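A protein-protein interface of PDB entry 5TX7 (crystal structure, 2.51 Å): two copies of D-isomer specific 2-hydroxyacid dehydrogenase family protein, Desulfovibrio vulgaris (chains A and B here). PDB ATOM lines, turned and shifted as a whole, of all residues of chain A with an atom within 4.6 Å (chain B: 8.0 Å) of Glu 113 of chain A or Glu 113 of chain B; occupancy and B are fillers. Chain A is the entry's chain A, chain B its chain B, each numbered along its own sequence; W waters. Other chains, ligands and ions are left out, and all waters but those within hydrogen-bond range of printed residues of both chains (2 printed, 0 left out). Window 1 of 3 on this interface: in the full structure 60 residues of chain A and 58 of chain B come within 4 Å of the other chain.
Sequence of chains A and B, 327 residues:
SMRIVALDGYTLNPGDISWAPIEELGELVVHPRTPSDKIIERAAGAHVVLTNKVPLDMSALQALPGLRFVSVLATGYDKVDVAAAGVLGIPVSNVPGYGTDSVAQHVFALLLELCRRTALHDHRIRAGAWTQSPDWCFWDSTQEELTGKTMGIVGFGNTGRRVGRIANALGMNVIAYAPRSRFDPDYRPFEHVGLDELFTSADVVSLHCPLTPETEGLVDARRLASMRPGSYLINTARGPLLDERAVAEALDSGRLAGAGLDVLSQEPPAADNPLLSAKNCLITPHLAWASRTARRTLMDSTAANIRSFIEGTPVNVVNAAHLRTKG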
ATOM      1  N   ALA A 109      19.995 -18.287  -5.647  1.00  0.00           N
ATOM      2  CA  ALA A 109      20.727 -18.200  -4.389  1.00  0.00           C
ATOM      3  C   ALA A 109      20.435 -16.854  -3.698  1.00  0.00           C
ATOM      4  O   ALA A 109      20.171 -16.813  -2.500  1.00  0.00           O
ATOM      5  CB  ALA A 109      22.212 -18.370  -4.612  1.00  0.00           C
ATOM      6  N   LEU A 110      20.439 -15.764  -4.453  1.00  0.00           N
ATOM      7  CA  LEU A 110      20.093 -14.441  -3.878  1.00  0.00           C
ATOM      8  C   LEU A 110      18.627 -14.392  -3.415  1.00  0.00           C
ATOM      9  O   LEU A 110      18.325 -13.975  -2.295  1.00  0.00           O
ATOM     10  CB  LEU A 110      20.343 -13.325  -4.890  1.00  0.00           C
ATOM     11  CG  LEU A 110      21.811 -13.102  -5.280  1.00  0.00           C
ATOM     12  CD1 LEU A 110      21.909 -12.281  -6.551  1.00  0.00           C
ATOM     13  CD2 LEU A 110      22.596 -12.401  -4.194  1.00  0.00           C
ATOM     14  N   LEU A 111      17.728 -14.845  -4.287  1.00  0.00           N
ATOM     15  CA  LEU A 111      16.295 -14.776  -4.021  1.00  0.00           C
ATOM     16  C   LEU A 111      15.855 -15.626  -2.828  1.00  0.00           C
ATOM     17  O   LEU A 111      15.018 -15.194  -2.038  1.00  0.00           O
ATOM     18  CB  LEU A 111      15.526 -15.195  -5.260  1.00  0.00           C
ATOM     19  CG  LEU A 111      14.000 -15.228  -5.190  1.00  0.00           C
ATOM     20  CD1 LEU A 111      13.511 -13.831  -4.846  1.00  0.00           C
ATOM     21  CD2 LEU A 111      13.438 -15.719  -6.501  1.00  0.00           C
ATOM     22  N   LEU A 112      16.391 -16.834  -2.711  1.00  0.00           N
ATOM     23  CA  LEU A 112      16.043 -17.723  -1.610  1.00  0.00           C
ATOM     24  C   LEU A 112      16.645 -17.307  -0.285  1.00  0.00           C
ATOM     25  O   LEU A 112      16.039 -17.561   0.763  1.00  0.00           O
ATOM     26  CB  LEU A 112      16.415 -19.177  -1.921  1.00  0.00           C
ATOM     27  CG  LEU A 112      15.502 -19.852  -2.937  1.00  0.00           C
ATOM     28  CD1 LEU A 112      16.109 -21.184  -3.359  1.00  0.00           C
ATOM     29  CD2 LEU A 112      14.119 -20.055  -2.362  1.00  0.00           C
ATOM     30  N   GLU A 113      17.809 -16.666  -0.318  1.00  0.00           N
ATOM     31  CA  GLU A 113      18.350 -16.076   0.897  1.00  0.00           C
ATOM     32  C   GLU A 113      17.482 -14.912   1.331  1.00  0.00           C
ATOM     33  O   GLU A 113      17.308 -14.738   2.533  1.00  0.00           O
ATOM     34  CB  GLU A 113      19.824 -15.680   0.755  1.00  0.00           C
ATOM     35  CG  GLU A 113      20.466 -15.041   1.996  1.00  0.00           C
ATOM     36  CD  GLU A 113      20.594 -15.910   3.246  1.00  0.00           C
ATOM     37  OE1 GLU A 113      20.551 -17.172   3.172  1.00  0.00           O
ATOM     38  OE2 GLU A 113      20.774 -15.283   4.336  1.00  0.00           O
ATOM     39  N   LEU A 114      16.941 -14.130   0.404  1.00  0.00           N
ATOM     40  CA  LEU A 114      15.998 -13.071   0.798  1.00  0.00           C
ATOM     41  C   LEU A 114      14.683 -13.680   1.369  1.00  0.00           C
ATOM     42  O   LEU A 114      14.100 -13.134   2.301  1.00  0.00           O
ATOM     43  CB  LEU A 114      15.691 -12.134  -0.364  1.00  0.00           C
ATOM     44  CG  LEU A 114      16.856 -11.263  -0.865  1.00  0.00           C
ATOM     45  CD1 LEU A 114      16.663 -10.752  -2.290  1.00  0.00           C
ATOM     46  CD2 LEU A 114      17.087 -10.080   0.061  1.00  0.00           C
ATOM     47  N   CYS A 115      14.237 -14.799   0.810  1.00  0.00           N
ATOM     48  CA  CYS A 115      12.959 -15.387   1.194  1.00  0.00           C
ATOM     49  C   CYS A 115      12.982 -16.209   2.478  1.00  0.00           C
ATOM     50  O   CYS A 115      12.012 -16.195   3.234  1.00  0.00           O
ATOM     51  CB  CYS A 115      12.386 -16.229   0.068  1.00  0.00           C
ATOM     52  SG  CYS A 115      11.837 -15.149  -1.277  1.00  0.00           S
ATOM     53  N   ARG A 116      14.090 -16.917   2.709  1.00  0.00           N
ATOM     54  CA  ARG A 116      14.259 -17.793   3.895  1.00  0.00           C
ATOM     55  C   ARG A 116      15.319 -17.300   4.880  1.00  0.00           C
ATOM     56  O   ARG A 116      15.239 -17.615   6.068  1.00  0.00           O
ATOM     57  CB  ARG A 116      14.636 -19.200   3.433  1.00  0.00           C
ATOM     58  CG  ARG A 116      13.812 -19.753   2.269  1.00  0.00           C
ATOM     59  CD  ARG A 116      12.333 -19.783   2.590  1.00  0.00           C
ATOM     60  NE  ARG A 116      12.009 -20.802   3.601  1.00  0.00           N
ATOM     61  CZ  ARG A 116      11.274 -21.896   3.418  1.00  0.00           C
ATOM     62  NH1 ARG A 116      10.731 -22.197   2.232  1.00  0.00           N
ATOM     63  NH2 ARG A 116      11.085 -22.708   4.454  1.00  0.00           N
ATOM     64  N   ARG A 117      16.317 -16.537   4.424  1.00  0.00           N
ATOM     65  CA  ARG A 117      17.365 -16.024   5.300  1.00  0.00           C
ATOM     66  C   ARG A 117      18.047 -17.162   6.054  1.00  0.00           C
ATOM     67  O   ARG A 117      18.182 -17.090   7.272  1.00  0.00           O
ATOM     68  CB  ARG A 117      16.793 -14.945   6.231  1.00  0.00           C
ATOM     69  CG  ARG A 117      16.400 -13.645   5.547  1.00  0.00           C
ATOM     70  CD  ARG A 117      17.622 -12.784   5.323  1.00  0.00           C
ATOM     71  NE  ARG A 117      17.322 -11.533   4.638  1.00  0.00           N
ATOM     72  CZ  ARG A 117      18.245 -10.671   4.176  1.00  0.00           C
ATOM     73  NH1 ARG A 117      19.559 -10.928   4.268  1.00  0.00           N
ATOM     74  NH2 ARG A 117      17.860  -9.543   3.580  1.00  0.00           N
ATOM     75  N   THR A 118      18.491 -18.200   5.334  1.00  0.00           N
ATOM     76  CA  THR A 118      19.055 -19.385   6.012  1.00  0.00           C
ATOM     77  C   THR A 118      20.293 -19.040   6.785  1.00  0.00           C
ATOM     78  O   THR A 118      20.471 -19.510   7.897  1.00  0.00           O
ATOM     79  CB  THR A 118      19.415 -20.531   5.070  1.00  0.00           C
ATOM     80  OG1 THR A 118      20.303 -20.052   4.063  1.00  0.00           O
ATOM     81  CG2 THR A 118      18.151 -21.125   4.452  1.00  0.00           C
ATOM     82  N   ALA A 119      21.149 -18.219   6.199  1.00  0.00           N
ATOM     83  CA  ALA A 119      22.415 -17.830   6.831  1.00  0.00           C
ATOM     84  C   ALA A 119      22.218 -16.962   8.070  1.00  0.00           C
ATOM     85  O   ALA A 119      22.993 -17.065   9.027  1.00  0.00           O
ATOM     86  CB  ALA A 119      23.311 -17.115   5.829  1.00  0.00           C
ATOM     87  N   LEU A 120      21.210 -16.100   8.046  1.00  0.00           N
ATOM     88  CA  LEU A 120      20.827 -15.351   9.247  1.00  0.00           C
ATOM     89  C   LEU A 120      20.458 -16.308  10.386  1.00  0.00           C
ATOM     90  O   LEU A 120      21.018 -16.233  11.457  1.00  0.00           O
ATOM     91  CB  LEU A 120      19.677 -14.386   8.964  1.00  0.00           C
ATOM     92  CG  LEU A 120      19.070 -13.674  10.177  1.00  0.00           C
ATOM     93  CD1 LEU A 120      20.119 -12.839  10.896  1.00  0.00           C
ATOM     94  CD2 LEU A 120      17.897 -12.796   9.763  1.00  0.00           C
ATOM     95  N   LEU A 282      20.851  -7.432  -0.396  1.00  0.00           N
ATOM     96  CA  LEU A 282      21.876  -8.462  -0.398  1.00  0.00           C
ATOM     97  C   LEU A 282      22.812  -8.215  -1.588  1.00  0.00           C
ATOM     98  O   LEU A 282      22.360  -8.058  -2.719  1.00  0.00           O
ATOM     99  CB  LEU A 282      21.219  -9.829  -0.507  1.00  0.00           C
ATOM    100  CG  LEU A 282      22.024 -11.064  -0.172  1.00  0.00           C
ATOM    101  CD1 LEU A 282      22.327 -11.064   1.308  1.00  0.00           C
ATOM    102  CD2 LEU A 282      21.222 -12.313  -0.546  1.00  0.00           C
ATOM    103  N   HIS B 106      13.052 -25.172   0.890  1.00  0.00           N
ATOM    104  CA  HIS B 106      14.076 -25.022   1.931  1.00  0.00           C
ATOM    105  C   HIS B 106      15.323 -25.885   1.683  1.00  0.00           C
ATOM    106  O   HIS B 106      16.438 -25.467   1.998  1.00  0.00           O
ATOM    107  CB  HIS B 106      13.501 -25.288   3.333  1.00  0.00           C
ATOM    108  CG  HIS B 106      14.357 -24.741   4.430  1.00  0.00           C
ATOM    109  ND1 HIS B 106      14.553 -23.391   4.605  1.00  0.00           N
ATOM    110  CD2 HIS B 106      15.092 -25.360   5.384  1.00  0.00           C
ATOM    111  CE1 HIS B 106      15.361 -23.200   5.631  1.00  0.00           C
ATOM    112  NE2 HIS B 106      15.708 -24.378   6.117  1.00  0.00           N
ATOM    113  N   VAL B 107      15.136 -27.077   1.116  1.00  0.00           N
ATOM    114  CA  VAL B 107      16.269 -27.947   0.692  1.00  0.00           C
ATOM    115  C   VAL B 107      17.212 -27.154  -0.241  1.00  0.00           C
ATOM    116  O   VAL B 107      18.429 -27.180  -0.064  1.00  0.00           O
ATOM    117  CB  VAL B 107      15.740 -29.237  -0.003  1.00  0.00           C
ATOM    118  CG1 VAL B 107      16.819 -29.974  -0.782  1.00  0.00           C
ATOM    119  CG2 VAL B 107      15.098 -30.157   1.024  1.00  0.00           C
ATOM    120  N   PHE B 108      16.630 -26.418  -1.191  1.00  0.00           N
ATOM    121  CA  PHE B 108      17.385 -25.600  -2.127  1.00  0.00           C
ATOM    122  C   PHE B 108      17.862 -24.262  -1.580  1.00  0.00           C
ATOM    123  O   PHE B 108      18.903 -23.744  -2.044  1.00  0.00           O
ATOM    124  CB  PHE B 108      16.641 -25.473  -3.471  1.00  0.00           C
ATOM    125  CG  PHE B 108      16.577 -26.773  -4.210  1.00  0.00           C
ATOM    126  CD1 PHE B 108      17.678 -27.230  -4.912  1.00  0.00           C
ATOM    127  CD2 PHE B 108      15.464 -27.594  -4.101  1.00  0.00           C
ATOM    128  CE1 PHE B 108      17.663 -28.472  -5.554  1.00  0.00           C
ATOM    129  CE2 PHE B 108      15.435 -28.834  -4.746  1.00  0.00           C
ATOM    130  CZ  PHE B 108      16.541 -29.266  -5.489  1.00  0.00           C
ATOM    131  N   ALA B 109      17.161 -23.703  -0.597  1.00  0.00           N
ATOM    132  CA  ALA B 109      17.684 -22.528   0.119  1.00  0.00           C
ATOM    133  C   ALA B 109      18.936 -22.921   0.882  1.00  0.00           C
ATOM    134  O   ALA B 109      19.921 -22.208   0.835  1.00  0.00           O
ATOM    135  CB  ALA B 109      16.659 -21.936   1.059  1.00  0.00           C
ATOM    136  N   LEU B 110      18.919 -24.071   1.558  1.00  0.00           N
ATOM    137  CA  LEU B 110      20.115 -24.554   2.264  1.00  0.00           C
ATOM    138  C   LEU B 110      21.239 -24.884   1.287  1.00  0.00           C
ATOM    139  O   LEU B 110      22.371 -24.459   1.475  1.00  0.00           O
ATOM    140  CB  LEU B 110      19.791 -25.802   3.099  1.00  0.00           C
ATOM    141  CG  LEU B 110      18.880 -25.595   4.293  1.00  0.00           C
ATOM    142  CD1 LEU B 110      18.328 -26.930   4.768  1.00  0.00           C
ATOM    143  CD2 LEU B 110      19.603 -24.877   5.426  1.00  0.00           C
ATOM    144  N   LEU B 111      20.917 -25.653   0.251  1.00  0.00           N
ATOM    145  CA  LEU B 111      21.913 -26.114  -0.710  1.00  0.00           C
ATOM    146  C   LEU B 111      22.605 -24.981  -1.486  1.00  0.00           C
ATOM    147  O   LEU B 111      23.809 -25.025  -1.684  1.00  0.00           O
ATOM    148  CB  LEU B 111      21.250 -27.060  -1.694  1.00  0.00           C
ATOM    149  CG  LEU B 111      22.121 -27.721  -2.733  1.00  0.00           C
ATOM    150  CD1 LEU B 111      23.307 -28.460  -2.115  1.00  0.00           C
ATOM    151  CD2 LEU B 111      21.232 -28.687  -3.521  1.00  0.00           C
ATOM    152  N   LEU B 112      21.837 -23.992  -1.924  1.00  0.00           N
ATOM    153  CA  LEU B 112      22.395 -22.873  -2.683  1.00  0.00           C
ATOM    154  C   LEU B 112      23.172 -21.894  -1.791  1.00  0.00           C
ATOM    155  O   LEU B 112      24.110 -21.253  -2.240  1.00  0.00           O
ATOM    156  CB  LEU B 112      21.314 -22.114  -3.461  1.00  0.00           C
ATOM    157  CG  LEU B 112      20.760 -22.867  -4.666  1.00  0.00           C
ATOM    158  CD1 LEU B 112      19.540 -22.180  -5.230  1.00  0.00           C
ATOM    159  CD2 LEU B 112      21.782 -23.032  -5.760  1.00  0.00           C
ATOM    160  N   GLU B 113      22.782 -21.771  -0.534  1.00  0.00           N
ATOM    161  CA  GLU B 113      23.584 -21.002   0.394  1.00  0.00           C
ATOM    162  C   GLU B 113      24.888 -21.703   0.714  1.00  0.00           C
ATOM    163  O   GLU B 113      25.897 -21.033   0.882  1.00  0.00           O
ATOM    164  CB  GLU B 113      22.834 -20.631   1.665  1.00  0.00           C
ATOM    165  CG  GLU B 113      23.567 -19.608   2.536  1.00  0.00           C
ATOM    166  CD  GLU B 113      23.730 -18.203   1.895  1.00  0.00           C
ATOM    167  OE1 GLU B 113      24.097 -17.287   2.620  1.00  0.00           O
ATOM    168  OE2 GLU B 113      23.493 -17.945   0.684  1.00  0.00           O
ATOM    169  N   LEU B 114      24.900 -23.029   0.744  1.00  0.00           N
ATOM    170  CA  LEU B 114      26.190 -23.749   0.847  1.00  0.00           C
ATOM    171  C   LEU B 114      27.039 -23.585  -0.409  1.00  0.00           C
ATOM    172  O   LEU B 114      28.264 -23.474  -0.304  1.00  0.00           O
ATOM    173  CB  LEU B 114      25.993 -25.249   1.098  1.00  0.00           C
ATOM    174  CG  LEU B 114      25.348 -25.696   2.396  1.00  0.00           C
ATOM    175  CD1 LEU B 114      24.844 -27.117   2.207  1.00  0.00           C
ATOM    176  CD2 LEU B 114      26.327 -25.565   3.540  1.00  0.00           C
ATOM    177  N   CYS B 115      26.396 -23.544  -1.581  1.00  0.00           N
ATOM    178  CA  CYS B 115      27.109 -23.474  -2.855  1.00  0.00           C
ATOM    179  C   CYS B 115      27.639 -22.089  -3.179  1.00  0.00           C
ATOM    180  O   CYS B 115      28.708 -22.001  -3.779  1.00  0.00           O
ATOM    181  CB  CYS B 115      26.205 -23.926  -4.004  1.00  0.00           C
ATOM    182  SG  CYS B 115      25.875 -25.688  -4.066  1.00  0.00           S
ATOM    183  N   ARG B 116      26.880 -21.043  -2.843  1.00  0.00           N
ATOM    184  CA  ARG B 116      27.226 -19.662  -3.138  1.00  0.00           C
ATOM    185  C   ARG B 116      27.597 -18.793  -1.906  1.00  0.00           C
ATOM    186  O   ARG B 116      28.394 -17.886  -2.031  1.00  0.00           O
ATOM    187  CB  ARG B 116      26.113 -18.978  -3.925  1.00  0.00           C
ATOM    188  CG  ARG B 116      25.475 -19.809  -5.032  1.00  0.00           C
ATOM    189  CD  ARG B 116      26.439 -20.312  -6.080  1.00  0.00           C
ATOM    190  NE  ARG B 116      27.073 -19.265  -6.885  1.00  0.00           N
ATOM    191  CZ  ARG B 116      26.845 -19.006  -8.177  1.00  0.00           C
ATOM    192  NH1 ARG B 116      25.936 -19.670  -8.890  1.00  0.00           N
ATOM    193  NH2 ARG B 116      27.547 -18.047  -8.782  1.00  0.00           N
ATOM    194  N   ARG B 117      27.022 -19.082  -0.744  1.00  0.00           N
ATOM    195  CA  ARG B 117      27.299 -18.324   0.480  1.00  0.00           C
ATOM    196  C   ARG B 117      27.084 -16.808   0.273  1.00  0.00           C
ATOM    197  O   ARG B 117      27.967 -15.991   0.576  1.00  0.00           O
ATOM    198  CB  ARG B 117      28.730 -18.581   0.988  1.00  0.00           C
ATOM    199  CG  ARG B 117      28.989 -19.977   1.516  1.00  0.00           C
ATOM    200  CD  ARG B 117      28.498 -20.061   2.934  1.00  0.00           C
ATOM    201  NE  ARG B 117      28.604 -21.404   3.495  1.00  0.00           N
ATOM    202  CZ  ARG B 117      28.255 -21.739   4.735  1.00  0.00           C
ATOM    203  NH1 ARG B 117      27.816 -20.814   5.592  1.00  0.00           N
ATOM    204  NH2 ARG B 117      28.382 -23.007   5.133  1.00  0.00           N
ATOM    205  N   THR B 118      25.907 -16.442  -0.246  1.00  0.00           N
ATOM    206  CA  THR B 118      25.609 -15.061  -0.557  1.00  0.00           C
ATOM    207  C   THR B 118      25.722 -14.149   0.653  1.00  0.00           C
ATOM    208  O   THR B 118      26.269 -13.064   0.542  1.00  0.00           O
ATOM    209  CB  THR B 118      24.204 -14.847  -1.138  1.00  0.00           C
ATOM    210  OG1 THR B 118      23.225 -15.376  -0.232  1.00  0.00           O
ATOM    211  CG2 THR B 118      24.077 -15.492  -2.495  1.00  0.00           C
ATOM    212  N   ALA B 119      25.203 -14.595   1.789  1.00  0.00           N
ATOM    213  CA  ALA B 119      25.185 -13.769   3.002  1.00  0.00           C
ATOM    214  C   ALA B 119      26.572 -13.535   3.582  1.00  0.00           C
ATOM    215  O   ALA B 119      26.844 -12.448   4.124  1.00  0.00           O
ATOM    216  CB  ALA B 119      24.281 -14.376   4.063  1.00  0.00           C
ATOM    217  N   LEU B 120      27.437 -14.546   3.479  1.00  0.00           N
ATOM    218  CA  LEU B 120      28.835 -14.377   3.848  1.00  0.00           C
ATOM    219  C   LEU B 120      29.474 -13.264   3.020  1.00  0.00           C
ATOM    220  O   LEU B 120      30.029 -12.319   3.572  1.00  0.00           O
ATOM    221  CB  LEU B 120      29.616 -15.689   3.682  1.00  0.00           C
ATOM    222  CG  LEU B 120      31.143 -15.617   3.780  1.00  0.00           C
ATOM    223  CD1 LEU B 120      31.549 -15.132   5.155  1.00  0.00           C
ATOM    224  CD2 LEU B 120      31.740 -16.973   3.498  1.00  0.00           C
ATOM    225  N   HIS B 121      29.375 -13.353   1.702  1.00  0.00           N
ATOM    226  CA  HIS B 121      29.995 -12.356   0.833  1.00  0.00           C
ATOM    227  C   HIS B 121      29.422 -10.957   0.987  1.00  0.00           C
ATOM    228  O   HIS B 121      30.144  -9.969   0.813  1.00  0.00           O
ATOM    229  CB  HIS B 121      29.918 -12.791  -0.627  1.00  0.00           C
ATOM    230  CG  HIS B 121      30.751 -13.980  -0.916  1.00  0.00           C
ATOM    231  ND1 HIS B 121      30.236 -15.251  -0.893  1.00  0.00           N
ATOM    232  CD2 HIS B 121      32.068 -14.109  -1.178  1.00  0.00           C
ATOM    233  CE1 HIS B 121      31.202 -16.118  -1.139  1.00  0.00           C
ATOM    234  NE2 HIS B 121      32.325 -15.449  -1.303  1.00  0.00           N
ATOM    235  N   ASP B 122      28.133 -10.877   1.291  1.00  0.00           N
ATOM    236  CA  ASP B 122      27.508  -9.605   1.664  1.00  0.00           C
ATOM    237  C   ASP B 122      28.158  -9.007   2.927  1.00  0.00           C
ATOM    238  O   ASP B 122      28.465  -7.813   2.971  1.00  0.00           O
ATOM    239  CB  ASP B 122      26.006  -9.802   1.852  1.00  0.00           C
ATOM    240  CG  ASP B 122      25.300  -8.555   2.316  1.00  0.00           C
ATOM    241  OD1 ASP B 122      24.936  -7.732   1.459  1.00  0.00           O
ATOM    242  OD2 ASP B 122      25.070  -8.423   3.540  1.00  0.00           O
ATOM    243  N   SER B 141      34.609 -18.301  -0.575  1.00  0.00           N
ATOM    244  CA  SER B 141      34.060 -19.643  -0.584  1.00  0.00           C
ATOM    245  C   SER B 141      33.847 -19.984  -2.037  1.00  0.00           C
ATOM    246  O   SER B 141      33.179 -19.233  -2.732  1.00  0.00           O
ATOM    247  CB  SER B 141      32.711 -19.656   0.154  1.00  0.00           C
ATOM    248  OG  SER B 141      32.397 -20.963   0.578  1.00  0.00           O
ATOM    249  N   THR B 142      34.406 -21.102  -2.490  1.00  0.00           N
ATOM    250  CA  THR B 142      34.241 -21.530  -3.870  1.00  0.00           C
ATOM    251  C   THR B 142      32.765 -21.556  -4.270  1.00  0.00           C
ATOM    252  O   THR B 142      31.929 -22.077  -3.537  1.00  0.00           O
ATOM    253  CB  THR B 142      34.880 -22.897  -4.125  1.00  0.00           C
ATOM    254  OG1 THR B 142      36.307 -22.781  -3.977  1.00  0.00           O
ATOM    255  CG2 THR B 142      34.586 -23.369  -5.548  1.00  0.00           C
ATOM    256  N   GLN B 143      32.472 -20.956  -5.423  1.00  0.00           N
ATOM    257  CA  GLN B 143      31.132 -20.926  -5.992  1.00  0.00           C
ATOM    258  C   GLN B 143      30.910 -22.263  -6.727  1.00  0.00           C
ATOM    259  O   GLN B 143      31.690 -22.677  -7.572  1.00  0.00           O
ATOM    260  CB  GLN B 143      30.949 -19.745  -6.939  1.00  0.00           C
ATOM    261  CG  GLN B 143      31.151 -18.391  -6.282  1.00  0.00           C
ATOM    262  CD  GLN B 143      30.134 -18.134  -5.177  1.00  0.00           C
ATOM    263  OE1 GLN B 143      28.995 -17.763  -5.430  1.00  0.00           O
ATOM    264  NE2 GLN B 143      30.543 -18.356  -3.945  1.00  0.00           N
ATOM    265  N   TYR B 232      27.414 -33.272  -0.955  1.00  0.00           N
ATOM    266  CA  TYR B 232      26.585 -32.442  -0.067  1.00  0.00           C
ATOM    267  C   TYR B 232      25.473 -33.274   0.570  1.00  0.00           C
ATOM    268  O   TYR B 232      24.927 -34.146  -0.092  1.00  0.00           O
ATOM    269  CB  TYR B 232      25.981 -31.272  -0.830  1.00  0.00           C
ATOM    270  CG  TYR B 232      26.987 -30.224  -1.258  1.00  0.00           C
ATOM    271  CD1 TYR B 232      27.692 -30.346  -2.460  1.00  0.00           C
ATOM    272  CD2 TYR B 232      27.199 -29.073  -0.498  1.00  0.00           C
ATOM    273  CE1 TYR B 232      28.610 -29.380  -2.863  1.00  0.00           C
ATOM    274  CE2 TYR B 232      28.105 -28.086  -0.907  1.00  0.00           C
ATOM    275  CZ  TYR B 232      28.797 -28.233  -2.100  1.00  0.00           C
ATOM    276  OH  TYR B 232      29.721 -27.289  -2.527  1.00  0.00           O
ATOM    277  N   LEU B 282      25.590 -25.659   7.479  1.00  0.00           N
ATOM    278  CA  LEU B 282      24.509 -24.686   7.624  1.00  0.00           C
ATOM    279  C   LEU B 282      23.344 -25.285   8.432  1.00  0.00           C
ATOM    280  O   LEU B 282      22.866 -26.360   8.104  1.00  0.00           O
ATOM    281  CB  LEU B 282      24.043 -24.246   6.242  1.00  0.00           C
ATOM    282  CG  LEU B 282      23.259 -22.926   6.163  1.00  0.00           C
ATOM    283  CD1 LEU B 282      24.053 -21.719   6.640  1.00  0.00           C
ATOM    284  CD2 LEU B 282      22.790 -22.681   4.746  1.00  0.00           C
ATOM    285  N   THR B 284      19.470 -24.509  10.373  1.00  0.00           N
ATOM    286  CA  THR B 284      18.295 -23.647  10.577  1.00  0.00           C
ATOM    287  C   THR B 284      17.388 -24.297  11.644  1.00  0.00           C
ATOM    288  O   THR B 284      17.375 -25.527  11.752  1.00  0.00           O
ATOM    289  CB  THR B 284      17.542 -23.405   9.248  1.00  0.00           C
ATOM    290  OG1 THR B 284      17.314 -24.646   8.589  1.00  0.00           O
ATOM    291  CG2 THR B 284      18.355 -22.511   8.336  1.00  0.00           C
HETATM  292  O   HOH W   1      21.647 -18.782  -1.266  1.00  0.00           O
HETATM  293  O   HOH W   2      19.366 -19.437  -0.113  1.00  0.00           O
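OE1 of Glu 113 of chain A sits at hydrogen-bond distance from N of Ala 119 of chain A (3.3 Å). The backbone NH (N) of Ala 119 of chain B sits at hydrogen-bond distance from the side-chain carboxylate (OE1) of Glu 113 of chain B. The side-chain amide oxygen of Gln 143 of chain B lies within hydrogen-bond range of the guanidinium group of Arg 116 of chain B.
Among the printed residues, merely in contact across the chains: Ala 119 of chain A with Glu 113 of chain B (3.3 Å), Ala 119 of chain A with Ala 119 of chain B (3.4 Å), Thr 118 of chain A with Glu 113 of chain B (3.5 Å), Arg 116 of chain A with His 106 of chain B (3.5 Å), Glu 113 of chain A with Thr 118 of chain B (3.6 Å), Glu 113 of chain A with Glu 113 of chain B (3.6 Å), Ala 109 of chain A with Arg 116 of chain B (3.6 Å), Glu 113 of chain A with Ala 119 of chain B (3.6 Å), Leu 282 of chain A with Asp 122 of chain B (3.7 Å), Thr 118 of chain A with His 106 of chain B (3.7 Å), Leu 282 of chain A with Thr 118 of chain B (3.7 Å), Thr 118 of chain A with Leu 282 of chain B (3.7 Å), Thr 118 of chain A with Thr 284 of chain B (3.7 Å), Arg 116 of chain A with Ala 109 of chain B (3.8 Å), Thr 118 of chain A with Ala 109 of chain B (3.8 Å), Leu 110 of chain A with Thr 118 of chain B (3.8 Å), Leu 112 of chain A with Ala 109 of chain B (3.9 Å), Ala 109 of chain A with Leu 112 of chain B (3.9 Å) and Leu 112 of chain A with Phe 108 of chain B (3.96 Å).
Glu 113 of chain A touches just these residues of chain B: Glu 113, Thr 118 and Ala 119. Glu 113 of chain B touches just these residues of chain A: Glu 113 (3.6 Å), Thr 118 (3.5 Å) and Ala 119 (3.3 Å). Printed residues of chain B within 4 Å of Thr 118 of chain A: His 106, Ala 109, Glu 113, Leu 282 and Thr 284. Of the printed residues of chain B, Leu 282 of chain A touches Thr 118 (3.7 Å) and Asp 122 (3.7 Å). Printed residues of chain B within 4 Å of Ala 119 of chain A: Glu 113 (3.3 Å) and Ala 119 (3.4 Å). Printed residues of chain A within 4 Å of Phe 108 of chain B: Leu 112 (3.96 Å). Ser 141 of chain B touches none of the printed residues of chain A. The nearest printed residue of chain A that does not touch Glu 113 of chain B is Ala 109 of chain A (4.7 Å).
Of the 13 printed residues of chain A, 8 touch a printed residue of chain B. Printed residues of chain A that touch a printed residue of chain B: Ala 109, Leu 110, Leu 112, Glu 113, Arg 116, Thr 118, Ala 119 and Leu 282. Hydrophobic or aromatic side chains of chain B that line the printed part of chain A: His 106, Ala 109, Leu 112, Ala 119 and Leu 282. Among the printed residues, 19 pairs touch across the chains. Among the printed residues, no Asp or Glu carboxylate lies within 4 Å of a Lys or Arg side-chain nitrogen of the other chain.
Glu 113 of chain A touches Thr 118 of chain B, and with the chains exchanged Thr 118 of chain A touches Glu 113 of chain B. Ala 119 of chain B touches its own counterpart, Ala 119 of chain A. Positions printed for both chains: 109, 110, 111, 112, 113, 114, 115, 116, 117, 118, 119, 120 and 282. Of the 19 pairs that touch across the chains among the printed residues, 12 have their exchanged pair printed and touching as well.
Water W1 lies within hydrogen-bond range of O of Ala 109 of chain A (2.8 Å) and OE2 of Glu 113 of chain B (2.8 Å). Water W2 lies within hydrogen-bond range of the backbone carbonyl oxygen (O) of Ala 109 of chain B (3.0 Å) and the backbone NH (N) of Glu 113 of chain A (3.2 Å).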
